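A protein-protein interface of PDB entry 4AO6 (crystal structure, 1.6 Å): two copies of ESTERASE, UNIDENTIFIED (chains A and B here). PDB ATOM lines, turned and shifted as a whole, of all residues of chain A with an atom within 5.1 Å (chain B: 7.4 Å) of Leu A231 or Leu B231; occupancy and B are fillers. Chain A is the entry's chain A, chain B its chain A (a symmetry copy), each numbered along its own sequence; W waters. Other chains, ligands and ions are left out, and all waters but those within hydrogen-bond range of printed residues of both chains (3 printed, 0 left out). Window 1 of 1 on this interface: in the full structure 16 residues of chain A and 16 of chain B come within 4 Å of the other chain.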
ATOM      1  N   TYR A 203      14.712 -15.168  30.819  1.00  0.00           N
ATOM      2  CA  TYR A 203      15.724 -14.088  30.789  1.00  0.00           C
ATOM      3  C   TYR A 203      15.168 -12.878  31.540  1.00  0.00           C
ATOM      4  O   TYR A 203      14.016 -12.485  31.338  1.00  0.00           O
ATOM      5  CB  TYR A 203      15.983 -13.728  29.322  1.00  0.00           C
ATOM      6  CG  TYR A 203      17.325 -13.115  29.078  1.00  0.00           C
ATOM      7  CD1 TYR A 203      17.523 -11.749  29.204  1.00  0.00           C
ATOM      8  CD2 TYR A 203      18.414 -13.928  28.719  1.00  0.00           C
ATOM      9  CE1 TYR A 203      18.795 -11.202  28.985  1.00  0.00           C
ATOM     10  CE2 TYR A 203      19.656 -13.402  28.495  1.00  0.00           C
ATOM     11  CZ  TYR A 203      19.850 -12.047  28.642  1.00  0.00           C
ATOM     12  OH  TYR A 203      21.125 -11.577  28.431  1.00  0.00           O
ATOM     13  N   LEU A 204      15.980 -12.307  32.435  1.00  0.00           N
ATOM     14  CA  LEU A 204      15.565 -11.135  33.218  1.00  0.00           C
ATOM     15  C   LEU A 204      16.331  -9.894  32.775  1.00  0.00           C
ATOM     16  O   LEU A 204      17.541  -9.939  32.560  1.00  0.00           O
ATOM     17  CB  LEU A 204      15.835 -11.350  34.739  1.00  0.00           C
ATOM     18  CG  LEU A 204      15.315 -12.632  35.390  1.00  0.00           C
ATOM     19  CD1 LEU A 204      15.605 -12.611  36.880  1.00  0.00           C
ATOM     20  CD2 LEU A 204      13.834 -12.764  35.135  1.00  0.00           C
ATOM     21  N   LEU A 205      15.612  -8.798  32.614  1.00  0.00           N
ATOM     22  CA  LEU A 205      16.268  -7.498  32.442  1.00  0.00           C
ATOM     23  C   LEU A 205      15.669  -6.447  33.352  1.00  0.00           C
ATOM     24  O   LEU A 205      14.504  -6.514  33.749  1.00  0.00           O
ATOM     25  CB  LEU A 205      16.136  -7.042  30.987  1.00  0.00           C
ATOM     26  CG  LEU A 205      16.929  -7.752  29.896  1.00  0.00           C
ATOM     27  CD1 LEU A 205      16.462  -7.139  28.575  1.00  0.00           C
ATOM     28  CD2 LEU A 205      18.449  -7.610  30.063  1.00  0.00           C
ATOM     29  N   TRP A 207      14.770  -2.444  33.628  1.00  0.00           N
ATOM     30  CA  TRP A 207      14.460  -1.355  32.685  1.00  0.00           C
ATOM     31  C   TRP A 207      15.510  -0.238  32.748  1.00  0.00           C
ATOM     32  O   TRP A 207      15.993   0.256  31.710  1.00  0.00           O
ATOM     33  CB  TRP A 207      13.072  -0.798  32.988  1.00  0.00           C
ATOM     34  CG  TRP A 207      12.561   0.152  31.918  1.00  0.00           C
ATOM     35  CD1 TRP A 207      12.793   1.500  31.821  1.00  0.00           C
ATOM     36  CD2 TRP A 207      11.720  -0.194  30.816  1.00  0.00           C
ATOM     37  NE1 TRP A 207      12.147   2.013  30.711  1.00  0.00           N
ATOM     38  CE2 TRP A 207      11.488   0.995  30.075  1.00  0.00           C
ATOM     39  CE3 TRP A 207      11.150  -1.398  30.374  1.00  0.00           C
ATOM     40  CZ2 TRP A 207      10.703   1.011  28.912  1.00  0.00           C
ATOM     41  CZ3 TRP A 207      10.363  -1.383  29.227  1.00  0.00           C
ATOM     42  CH2 TRP A 207      10.150  -0.181  28.511  1.00  0.00           C
ATOM     43  N   LEU A 218      17.720  -6.551  25.110  1.00  0.00           N
ATOM     44  CA  LEU A 218      16.768  -7.024  24.114  1.00  0.00           C
ATOM     45  C   LEU A 218      17.455  -7.678  22.918  1.00  0.00           C
ATOM     46  O   LEU A 218      17.049  -8.756  22.470  1.00  0.00           O
ATOM     47  CB  LEU A 218      15.852  -5.874  23.661  1.00  0.00           C
ATOM     48  CG  LEU A 218      14.892  -5.348  24.731  1.00  0.00           C
ATOM     49  CD1 LEU A 218      14.298  -3.991  24.348  1.00  0.00           C
ATOM     50  CD2 LEU A 218      13.779  -6.360  25.004  1.00  0.00           C
ATOM     51  N   PHE A 221      18.645 -11.203  23.993  1.00  0.00           N
ATOM     52  CA  PHE A 221      17.481 -12.071  24.097  1.00  0.00           C
ATOM     53  C   PHE A 221      16.940 -12.510  22.713  1.00  0.00           C
ATOM     54  O   PHE A 221      16.642 -13.692  22.494  1.00  0.00           O
ATOM     55  CB  PHE A 221      16.392 -11.389  24.929  1.00  0.00           C
ATOM     56  CG  PHE A 221      15.160 -12.209  25.068  1.00  0.00           C
ATOM     57  CD1 PHE A 221      15.101 -13.229  26.014  1.00  0.00           C
ATOM     58  CD2 PHE A 221      14.075 -12.021  24.198  1.00  0.00           C
ATOM     59  CE1 PHE A 221      13.959 -14.037  26.147  1.00  0.00           C
ATOM     60  CE2 PHE A 221      12.913 -12.829  24.314  1.00  0.00           C
ATOM     61  CZ  PHE A 221      12.858 -13.834  25.296  1.00  0.00           C
ATOM     62  N   LYS A 229      11.581 -19.374  25.015  1.00  0.00           N
ATOM     63  CA  LYS A 229      12.250 -18.335  25.832  1.00  0.00           C
ATOM     64  C   LYS A 229      11.217 -17.302  26.236  1.00  0.00           C
ATOM     65  O   LYS A 229      10.314 -16.998  25.476  1.00  0.00           O
ATOM     66  CB  LYS A 229      13.408 -17.676  25.075  1.00  0.00           C
ATOM     67  CG  LYS A 229      13.012 -17.054  23.722  1.00  0.00           C
ATOM     68  CD  LYS A 229      14.218 -16.459  22.981  1.00  0.00           C
ATOM     69  CE  LYS A 229      13.747 -15.881  21.670  1.00  0.00           C
ATOM     70  NZ  LYS A 229      14.897 -15.418  20.827  1.00  0.00           N
ATOM     71  N   THR A 230      11.367 -16.749  27.437  1.00  0.00           N
ATOM     72  CA  THR A 230      10.482 -15.688  27.893  1.00  0.00           C
ATOM     73  C   THR A 230      11.338 -14.633  28.590  1.00  0.00           C
ATOM     74  O   THR A 230      12.259 -14.991  29.325  1.00  0.00           O
ATOM     75  CB  THR A 230       9.440 -16.216  28.911  1.00  0.00           C
ATOM     76  OG1 THR A 230       8.657 -17.229  28.288  1.00  0.00           O
ATOM     77  CG2 THR A 230       8.493 -15.130  29.215  1.00  0.00           C
ATOM     78  N   LEU A 231      11.045 -13.366  28.317  1.00  0.00           N
ATOM     79  CA  LEU A 231      11.786 -12.226  28.891  1.00  0.00           C
ATOM     80  C   LEU A 231      10.895 -11.589  29.936  1.00  0.00           C
ATOM     81  O   LEU A 231       9.733 -11.340  29.658  1.00  0.00           O
ATOM     82  CB  LEU A 231      12.110 -11.170  27.808  1.00  0.00           C
ATOM     83  CG  LEU A 231      12.706  -9.872  28.326  1.00  0.00           C
ATOM     84  CD1 LEU A 231      14.101 -10.072  28.901  1.00  0.00           C
ATOM     85  CD2 LEU A 231      12.800  -8.847  27.171  1.00  0.00           C
ATOM     86  N   HIS A 232      11.433 -11.351  31.147  1.00  0.00           N
ATOM     87  CA  HIS A 232      10.717 -10.556  32.169  1.00  0.00           C
ATOM     88  C   HIS A 232      11.520  -9.303  32.389  1.00  0.00           C
ATOM     89  O   HIS A 232      12.738  -9.372  32.632  1.00  0.00           O
ATOM     90  CB  HIS A 232      10.668 -11.311  33.491  1.00  0.00           C
ATOM     91  CG  HIS A 232       9.766 -12.504  33.466  1.00  0.00           C
ATOM     92  ND1 HIS A 232       9.451 -13.204  34.608  1.00  0.00           N
ATOM     93  CD2 HIS A 232       9.091 -13.114  32.456  1.00  0.00           C
ATOM     94  CE1 HIS A 232       8.637 -14.203  34.307  1.00  0.00           C
ATOM     95  NE2 HIS A 232       8.395 -14.165  33.005  1.00  0.00           N
ATOM     96  N   VAL A 233      10.847  -8.176  32.282  1.00  0.00           N
ATOM     97  CA  VAL A 233      11.514  -6.873  32.502  1.00  0.00           C
ATOM     98  C   VAL A 233      10.824  -6.175  33.653  1.00  0.00           C
ATOM     99  O   VAL A 233       9.598  -6.046  33.659  1.00  0.00           O
ATOM    100  CB  VAL A 233      11.424  -5.963  31.292  1.00  0.00           C
ATOM    101  CG1 VAL A 233      12.365  -4.738  31.520  1.00  0.00           C
ATOM    102  CG2 VAL A 233      11.870  -6.690  30.031  1.00  0.00           C
ATOM    103  N   LEU B 177      -2.611  -6.385  31.301  1.00  0.00           N
ATOM    104  CA  LEU B 177      -2.737  -5.628  30.041  1.00  0.00           C
ATOM    105  C   LEU B 177      -1.756  -6.207  29.049  1.00  0.00           C
ATOM    106  O   LEU B 177      -0.928  -7.059  29.392  1.00  0.00           O
ATOM    107  CB  LEU B 177      -2.448  -4.131  30.272  1.00  0.00           C
ATOM    108  CG  LEU B 177      -3.411  -3.393  31.230  1.00  0.00           C
ATOM    109  CD1 LEU B 177      -2.828  -2.029  31.680  1.00  0.00           C
ATOM    110  CD2 LEU B 177      -4.818  -3.260  30.666  1.00  0.00           C
ATOM    111  N   GLY B 178      -1.868  -5.794  27.790  1.00  0.00           N
ATOM    112  CA  GLY B 178      -0.872  -6.240  26.844  1.00  0.00           C
ATOM    113  C   GLY B 178      -1.318  -6.214  25.409  1.00  0.00           C
ATOM    114  O   GLY B 178      -2.448  -5.797  25.089  1.00  0.00           O
ATOM    115  N   LEU B 179      -0.367  -6.580  24.550  1.00  0.00           N
ATOM    116  CA  LEU B 179      -0.592  -6.639  23.081  1.00  0.00           C
ATOM    117  C   LEU B 179      -1.113  -5.333  22.485  1.00  0.00           C
ATOM    118  O   LEU B 179      -2.001  -5.343  21.615  1.00  0.00           O
ATOM    119  CB  LEU B 179      -1.562  -7.786  22.731  1.00  0.00           C
ATOM    120  CG  LEU B 179      -1.225  -9.181  23.236  1.00  0.00           C
ATOM    121  CD1 LEU B 179      -2.176 -10.174  22.599  1.00  0.00           C
ATOM    122  CD2 LEU B 179       0.214  -9.612  22.976  1.00  0.00           C
ATOM    123  N   VAL B 201       0.606  -3.896  37.688  1.00  0.00           N
ATOM    124  CA  VAL B 201       0.301  -4.297  36.316  1.00  0.00           C
ATOM    125  C   VAL B 201       1.236  -5.410  35.909  1.00  0.00           C
ATOM    126  O   VAL B 201       2.461  -5.363  36.146  1.00  0.00           O
ATOM    127  CB  VAL B 201       0.520  -3.141  35.338  1.00  0.00           C
ATOM    128  CG1 VAL B 201       0.384  -3.595  33.877  1.00  0.00           C
ATOM    129  CG2 VAL B 201      -0.471  -2.023  35.649  1.00  0.00           C
ATOM    130  N   ARG B 202       0.677  -6.418  35.244  1.00  0.00           N
ATOM    131  CA  ARG B 202       1.503  -7.310  34.443  1.00  0.00           C
ATOM    132  C   ARG B 202       1.111  -7.014  33.000  1.00  0.00           C
ATOM    133  O   ARG B 202      -0.061  -6.970  32.677  1.00  0.00           O
ATOM    134  CB  ARG B 202       1.240  -8.800  34.761  1.00  0.00           C
ATOM    135  CG  ARG B 202       2.049  -9.699  33.798  1.00  0.00           C
ATOM    136  CD  ARG B 202       1.873 -11.163  34.088  1.00  0.00           C
ATOM    137  NE  ARG B 202       2.554 -11.539  35.316  1.00  0.00           N
ATOM    138  CZ  ARG B 202       2.588 -12.786  35.773  1.00  0.00           C
ATOM    139  NH1 ARG B 202       1.997 -13.761  35.072  1.00  0.00           N
ATOM    140  NH2 ARG B 202       3.217 -13.045  36.915  1.00  0.00           N
ATOM    141  N   TYR B 203       2.113  -6.837  32.151  1.00  0.00           N
ATOM    142  CA  TYR B 203       1.913  -6.456  30.735  1.00  0.00           C
ATOM    143  C   TYR B 203       2.545  -7.530  29.849  1.00  0.00           C
ATOM    144  O   TYR B 203       3.674  -7.965  30.091  1.00  0.00           O
ATOM    145  CB  TYR B 203       2.605  -5.108  30.508  1.00  0.00           C
ATOM    146  CG  TYR B 203       2.040  -4.323  29.367  1.00  0.00           C
ATOM    147  CD1 TYR B 203       2.499  -4.510  28.072  1.00  0.00           C
ATOM    148  CD2 TYR B 203       1.024  -3.381  29.598  1.00  0.00           C
ATOM    149  CE1 TYR B 203       1.941  -3.773  27.018  1.00  0.00           C
ATOM    150  CE2 TYR B 203       0.481  -2.651  28.577  1.00  0.00           C
ATOM    151  CZ  TYR B 203       0.926  -2.856  27.291  1.00  0.00           C
ATOM    152  OH  TYR B 203       0.325  -2.114  26.301  1.00  0.00           O
ATOM    153  N   LEU B 204       1.799  -7.983  28.836  1.00  0.00           N
ATOM    154  CA  LEU B 204       2.294  -9.011  27.910  1.00  0.00           C
ATOM    155  C   LEU B 204       2.550  -8.413  26.532  1.00  0.00           C
ATOM    156  O   LEU B 204       1.750  -7.635  26.019  1.00  0.00           O
ATOM    157  CB  LEU B 204       1.261 -10.167  27.749  1.00  0.00           C
ATOM    158  CG  LEU B 204       0.704 -10.820  29.015  1.00  0.00           C
ATOM    159  CD1 LEU B 204      -0.214 -11.971  28.644  1.00  0.00           C
ATOM    160  CD2 LEU B 204       1.844 -11.302  29.878  1.00  0.00           C
ATOM    161  N   LEU B 205       3.685  -8.763  25.953  1.00  0.00           N
ATOM    162  CA  LEU B 205       3.921  -8.461  24.537  1.00  0.00           C
ATOM    163  C   LEU B 205       4.430  -9.673  23.786  1.00  0.00           C
ATOM    164  O   LEU B 205       5.057 -10.573  24.348  1.00  0.00           O
ATOM    165  CB  LEU B 205       4.939  -7.325  24.414  1.00  0.00           C
ATOM    166  CG  LEU B 205       4.540  -5.906  24.802  1.00  0.00           C
ATOM    167  CD1 LEU B 205       5.815  -5.068  24.686  1.00  0.00           C
ATOM    168  CD2 LEU B 205       3.420  -5.330  23.924  1.00  0.00           C
ATOM    169  N   GLN B 206       4.156  -9.693  22.482  1.00  0.00           N
ATOM    170  CA  GLN B 206       4.651 -10.749  21.606  1.00  0.00           C
ATOM    171  C   GLN B 206       5.761 -10.178  20.740  1.00  0.00           C
ATOM    172  O   GLN B 206       5.592  -9.141  20.139  1.00  0.00           O
ATOM    173  CB  GLN B 206       3.506 -11.271  20.727  1.00  0.00           C
ATOM    174  CG  GLN B 206       2.542 -12.162  21.506  1.00  0.00           C
ATOM    175  CD  GLN B 206       3.201 -13.451  21.902  1.00  0.00           C
ATOM    176  OE1 GLN B 206       3.446 -13.712  23.072  1.00  0.00           O
ATOM    177  NE2 GLN B 206       3.517 -14.290  20.894  1.00  0.00           N
ATOM    178  N   TRP B 207       6.898 -10.858  20.718  1.00  0.00           N
ATOM    179  CA  TRP B 207       8.106 -10.331  20.060  1.00  0.00           C
ATOM    180  C   TRP B 207       7.852 -10.018  18.579  1.00  0.00           C
ATOM    181  O   TRP B 207       8.239  -8.949  18.068  1.00  0.00           O
ATOM    182  CB  TRP B 207       9.244 -11.339  20.203  1.00  0.00           C
ATOM    183  CG  TRP B 207      10.593 -10.782  19.781  1.00  0.00           C
ATOM    184  CD1 TRP B 207      11.125 -10.757  18.516  1.00  0.00           C
ATOM    185  CD2 TRP B 207      11.569 -10.194  20.641  1.00  0.00           C
ATOM    186  NE1 TRP B 207      12.380 -10.176  18.542  1.00  0.00           N
ATOM    187  CE2 TRP B 207      12.672  -9.817  19.831  1.00  0.00           C
ATOM    188  CE3 TRP B 207      11.613  -9.935  22.020  1.00  0.00           C
ATOM    189  CZ2 TRP B 207      13.813  -9.194  20.361  1.00  0.00           C
ATOM    190  CZ3 TRP B 207      12.746  -9.327  22.550  1.00  0.00           C
ATOM    191  CH2 TRP B 207      13.831  -8.964  21.715  1.00  0.00           C
ATOM    192  N   LEU B 214       7.100  -4.321  18.646  1.00  0.00           N
ATOM    193  CA  LEU B 214       7.682  -4.483  19.972  1.00  0.00           C
ATOM    194  C   LEU B 214       8.064  -3.122  20.564  1.00  0.00           C
ATOM    195  O   LEU B 214       7.743  -2.846  21.719  1.00  0.00           O
ATOM    196  CB  LEU B 214       8.882  -5.410  19.915  1.00  0.00           C
ATOM    197  CG  LEU B 214       9.560  -5.673  21.265  1.00  0.00           C
ATOM    198  CD1 LEU B 214       8.671  -6.503  22.202  1.00  0.00           C
ATOM    199  CD2 LEU B 214      10.864  -6.370  20.989  1.00  0.00           C
ATOM    200  N   GLY B 217       5.133  -1.226  21.876  1.00  0.00           N
ATOM    201  CA  GLY B 217       4.654  -1.869  23.103  1.00  0.00           C
ATOM    202  C   GLY B 217       5.541  -1.497  24.276  1.00  0.00           C
ATOM    203  O   GLY B 217       5.044  -1.150  25.341  1.00  0.00           O
ATOM    204  N   LEU B 218       6.850  -1.536  24.067  1.00  0.00           N
ATOM    205  CA  LEU B 218       7.794  -1.077  25.077  1.00  0.00           C
ATOM    206  C   LEU B 218       7.551   0.375  25.483  1.00  0.00           C
ATOM    207  O   LEU B 218       7.539   0.703  26.674  1.00  0.00           O
ATOM    208  CB  LEU B 218       9.239  -1.276  24.587  1.00  0.00           C
ATOM    209  CG  LEU B 218       9.679  -2.734  24.442  1.00  0.00           C
ATOM    210  CD1 LEU B 218      10.956  -2.865  23.608  1.00  0.00           C
ATOM    211  CD2 LEU B 218       9.870  -3.382  25.814  1.00  0.00           C
ATOM    212  N   PHE B 221       4.452   0.472  27.805  1.00  0.00           N
ATOM    213  CA  PHE B 221       4.830  -0.073  29.100  1.00  0.00           C
ATOM    214  C   PHE B 221       5.678   0.918  29.939  1.00  0.00           C
ATOM    215  O   PHE B 221       5.428   1.113  31.136  1.00  0.00           O
ATOM    216  CB  PHE B 221       5.556  -1.407  28.916  1.00  0.00           C
ATOM    217  CG  PHE B 221       5.990  -2.022  30.198  1.00  0.00           C
ATOM    218  CD1 PHE B 221       5.083  -2.739  30.974  1.00  0.00           C
ATOM    219  CD2 PHE B 221       7.292  -1.820  30.683  1.00  0.00           C
ATOM    220  CE1 PHE B 221       5.460  -3.306  32.204  1.00  0.00           C
ATOM    221  CE2 PHE B 221       7.692  -2.382  31.924  1.00  0.00           C
ATOM    222  CZ  PHE B 221       6.771  -3.130  32.679  1.00  0.00           C
ATOM    223  N   GLY B 222       6.666   1.543  29.304  1.00  0.00           N
ATOM    224  CA  GLY B 222       7.507   2.512  30.001  1.00  0.00           C
ATOM    225  C   GLY B 222       6.737   3.686  30.582  1.00  0.00           C
ATOM    226  O   GLY B 222       7.131   4.236  31.618  1.00  0.00           O
ATOM    227  N   LYS B 229       5.148  -2.802  38.125  1.00  0.00           N
ATOM    228  CA  LYS B 229       4.772  -3.316  36.788  1.00  0.00           C
ATOM    229  C   LYS B 229       5.833  -4.299  36.334  1.00  0.00           C
ATOM    230  O   LYS B 229       7.005  -4.119  36.614  1.00  0.00           O
ATOM    231  CB  LYS B 229       4.611  -2.183  35.769  1.00  0.00           C
ATOM    232  CG  LYS B 229       5.853  -1.284  35.615  1.00  0.00           C
ATOM    233  CD  LYS B 229       5.618  -0.134  34.626  1.00  0.00           C
ATOM    234  CE  LYS B 229       6.873   0.698  34.540  1.00  0.00           C
ATOM    235  NZ  LYS B 229       6.665   1.927  33.707  1.00  0.00           N
ATOM    236  N   THR B 230       5.413  -5.335  35.612  1.00  0.00           N
ATOM    237  CA  THR B 230       6.355  -6.294  35.054  1.00  0.00           C
ATOM    238  C   THR B 230       5.907  -6.616  33.631  1.00  0.00           C
ATOM    239  O   THR B 230       4.708  -6.758  33.393  1.00  0.00           O
ATOM    240  CB  THR B 230       6.369  -7.613  35.867  1.00  0.00           C
ATOM    241  OG1 THR B 230       6.749  -7.325  37.209  1.00  0.00           O
ATOM    242  CG2 THR B 230       7.441  -8.474  35.340  1.00  0.00           C
ATOM    243  N   LEU B 231       6.868  -6.683  32.716  1.00  0.00           N
ATOM    244  CA  LEU B 231       6.605  -6.964  31.291  1.00  0.00           C
ATOM    245  C   LEU B 231       7.061  -8.382  31.019  1.00  0.00           C
ATOM    246  O   LEU B 231       8.164  -8.738  31.403  1.00  0.00           O
ATOM    247  CB  LEU B 231       7.402  -6.005  30.377  1.00  0.00           C
ATOM    248  CG  LEU B 231       7.348  -6.329  28.892  1.00  0.00           C
ATOM    249  CD1 LEU B 231       5.957  -6.123  28.312  1.00  0.00           C
ATOM    250  CD2 LEU B 231       8.333  -5.415  28.125  1.00  0.00           C
ATOM    251  N   HIS B 232       6.201  -9.199  30.381  1.00  0.00           N
ATOM    252  CA  HIS B 232       6.618 -10.532  29.892  1.00  0.00           C
ATOM    253  C   HIS B 232       6.534 -10.491  28.391  1.00  0.00           C
ATOM    254  O   HIS B 232       5.496 -10.101  27.829  1.00  0.00           O
ATOM    255  CB  HIS B 232       5.651 -11.603  30.379  1.00  0.00           C
ATOM    256  CG  HIS B 232       5.742 -11.866  31.850  1.00  0.00           C
ATOM    257  ND1 HIS B 232       5.082 -12.919  32.443  1.00  0.00           N
ATOM    258  CD2 HIS B 232       6.425 -11.243  32.846  1.00  0.00           C
ATOM    259  CE1 HIS B 232       5.336 -12.926  33.742  1.00  0.00           C
ATOM    260  NE2 HIS B 232       6.158 -11.923  34.012  1.00  0.00           N
ATOM    261  N   VAL B 233       7.625 -10.869  27.756  1.00  0.00           N
ATOM    262  CA  VAL B 233       7.664 -10.901  26.276  1.00  0.00           C
ATOM    263  C   VAL B 233       7.953 -12.320  25.840  1.00  0.00           C
ATOM    264  O   VAL B 233       8.908 -12.938  26.317  1.00  0.00           O
ATOM    265  CB  VAL B 233       8.755 -10.014  25.705  1.00  0.00           C
ATOM    266  CG1 VAL B 233       8.553  -9.911  24.160  1.00  0.00           C
ATOM    267  CG2 VAL B 233       8.683  -8.615  26.299  1.00  0.00           C
ATOM    268  N   ASN B 234       7.123 -12.828  24.921  1.00  0.00           N
ATOM    269  CA  ASN B 234       7.322 -14.160  24.360  1.00  0.00           C
ATOM    270  C   ASN B 234       7.453 -14.074  22.855  1.00  0.00           C
ATOM    271  O   ASN B 234       6.940 -13.147  22.268  1.00  0.00           O
ATOM    272  CB  ASN B 234       6.136 -15.065  24.704  1.00  0.00           C
ATOM    273  CG  ASN B 234       6.096 -15.407  26.186  1.00  0.00           C
ATOM    274  OD1 ASN B 234       6.802 -16.298  26.626  1.00  0.00           O
ATOM    275  ND2 ASN B 234       5.234 -14.735  26.925  1.00  0.00           N
ATOM    276  N   PRO B 235       8.130 -15.055  22.254  1.00  0.00           N
ATOM    277  CA  PRO B 235       8.238 -15.080  20.785  1.00  0.00           C
ATOM    278  C   PRO B 235       6.901 -15.318  20.122  1.00  0.00           C
ATOM    279  O   PRO B 235       5.996 -15.912  20.715  1.00  0.00           O
ATOM    280  CB  PRO B 235       9.128 -16.293  20.502  1.00  0.00           C
ATOM    281  CG  PRO B 235       9.789 -16.642  21.770  1.00  0.00           C
ATOM    282  CD  PRO B 235       8.899 -16.151  22.888  1.00  0.00           C
ATOM    283  N   GLU B 245       1.013 -18.809  29.636  1.00  0.00           N
ATOM    284  CA  GLU B 245       1.137 -17.387  29.968  1.00  0.00           C
ATOM    285  C   GLU B 245      -0.269 -16.773  29.978  1.00  0.00           C
ATOM    286  O   GLU B 245      -0.658 -16.078  30.951  1.00  0.00           O
ATOM    287  CB  GLU B 245       2.066 -16.701  28.952  1.00  0.00           C
ATOM    288  CG  GLU B 245       2.326 -15.202  29.214  1.00  0.00           C
ATOM    289  CD  GLU B 245       3.483 -14.994  30.204  1.00  0.00           C
ATOM    290  OE1 GLU B 245       4.683 -15.133  29.827  1.00  0.00           O
ATOM    291  OE2 GLU B 245       3.199 -14.749  31.396  1.00  0.00           O
HETATM  292  O   HOH W   1       7.884 -18.598  25.292  1.00  0.00           O
HETATM  293  O   HOH W   2       7.100 -11.609  36.639  1.00  0.00           O
HETATM  294  O   HOH W   3       6.595 -16.019  31.905  1.00  0.00           O
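The side-chain amide oxygen (OD1) of Asn B234 sits at hydrogen-bond distance from the side-chain hydroxyl (OG1) of Thr A230 (2.7 Å). N of Val B233 sits at hydrogen-bond distance from O of Leu A231 (2.9 Å). A ring nitrogen (NE2) of His B232 is in hydrogen-bond range of a ring nitrogen (NE2) of His A232 (3.3 Å). The backbone NH (N) of Val A233 lies within hydrogen-bond range of the backbone carbonyl oxygen (O) of Leu B231.
N of Tyr A203 is in hydrogen-bond range of O of Thr A230 (2.9 Å). The backbone NH (N) of His A232 lies within hydrogen-bond range of the backbone carbonyl oxygen (O) of Tyr A203. The backbone carbonyl oxygen (O) of Val B201 lies within hydrogen-bond range of the backbone NH (N) of Thr B230 (3.0 Å). The backbone NH of Trp B207 lies within hydrogen-bond range of the backbone carbonyl oxygen of Asn B234, at 2.8 Å. O of Gly B222 lies within hydrogen-bond range of NZ of Lys B229, at 3.1 Å. ND2 of Asn B234 lies within hydrogen-bond range of OE1 of Glu B245 (3.0 Å).
CZ2 of Trp A207 touches CA of Gly B222, at 3.7 Å. Trp B207 touches Leu A218 (CH2 to O, 3.3 Å). OD1 of Asn B234 touches O of Lys A229 (3.8 Å). Lys A229 touches Pro B235 (O to CD, 3.1 Å). Thr A230 touches Val B233 (CA to O, 3.5 Å). Thr A230 touches Glu B245 (CG2 to OE1, 3.9 Å). O of Leu B231 touches O of Leu A231 (3.5 Å). Leu A231 touches His B232. Leu B231 touches His A232 (O to CA, 3.2 Å). Val A233 touches Thr B230 (O to CA, 3.5 Å).
Leu A231 touches three residues of chain B. Printed residues of chain A within 4 Å of Trp B207: Leu A218 (3.3 Å) and Phe A221 (3.4 Å). Of the printed residues of chain B, Lys A229 touches Asn B234 (3.8 Å) and Pro B235 (3.1 Å). Of the printed residues of chain A, Glu B245 touches Thr A230 (3.9 Å). Printed residues of chain A within 4 Å of Phe B221: Trp A207. Of the printed residues of chain B, Trp A207 touches Leu B218, Phe B221 and Gly B222. Leu B177 touches none of the printed residues of chain A. Leu B179 touches none of the printed residues of chain A. The nearest printed residue of chain B that does not touch Val A233 is Phe B221 (4.2 Å).
Hydrophobic or aromatic side chains of chain A within 4 Å of the printed part of chain B: Trp A207, Leu A218, Phe A221, Leu A231 and His A232. Among the printed residues, no Asp or Glu carboxylate lies within 4 Å of a Lys or Arg side-chain nitrogen of the other chain.
Trp A207 touches Phe B221, and with the chains exchanged Phe A221 touches Trp B207. Leu B218 touches its own counterpart, Leu A218. Thr A230 touches Val B233, and with the chains exchanged Val A233 touches Thr B230. Leu B231 touches its own counterpart, Leu A231. Positions printed for both chains: 203, 204, 205, 207, 218, 221, 229, 230, 231, 232 and 233. Of the 18 pairs that touch across the chains among the printed residues, 13 have their exchanged pair printed and touching as well.
Water W3 lies within hydrogen-bond range of NE2 of His A232, OE1 of Glu B245 and ND1 of His B232. Water W2 lies within hydrogen-bond range of a ring nitrogen (NE2) of His B232 (2.8 Å) and a ring nitrogen (ND1) of His A232 (3.5 Å). Water W1 lies within hydrogen-bond range of the side-chain amide oxygen of Asn B234, the backbone carbonyl oxygen of Lys A229 and the side-chain hydroxyl of Thr A230.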
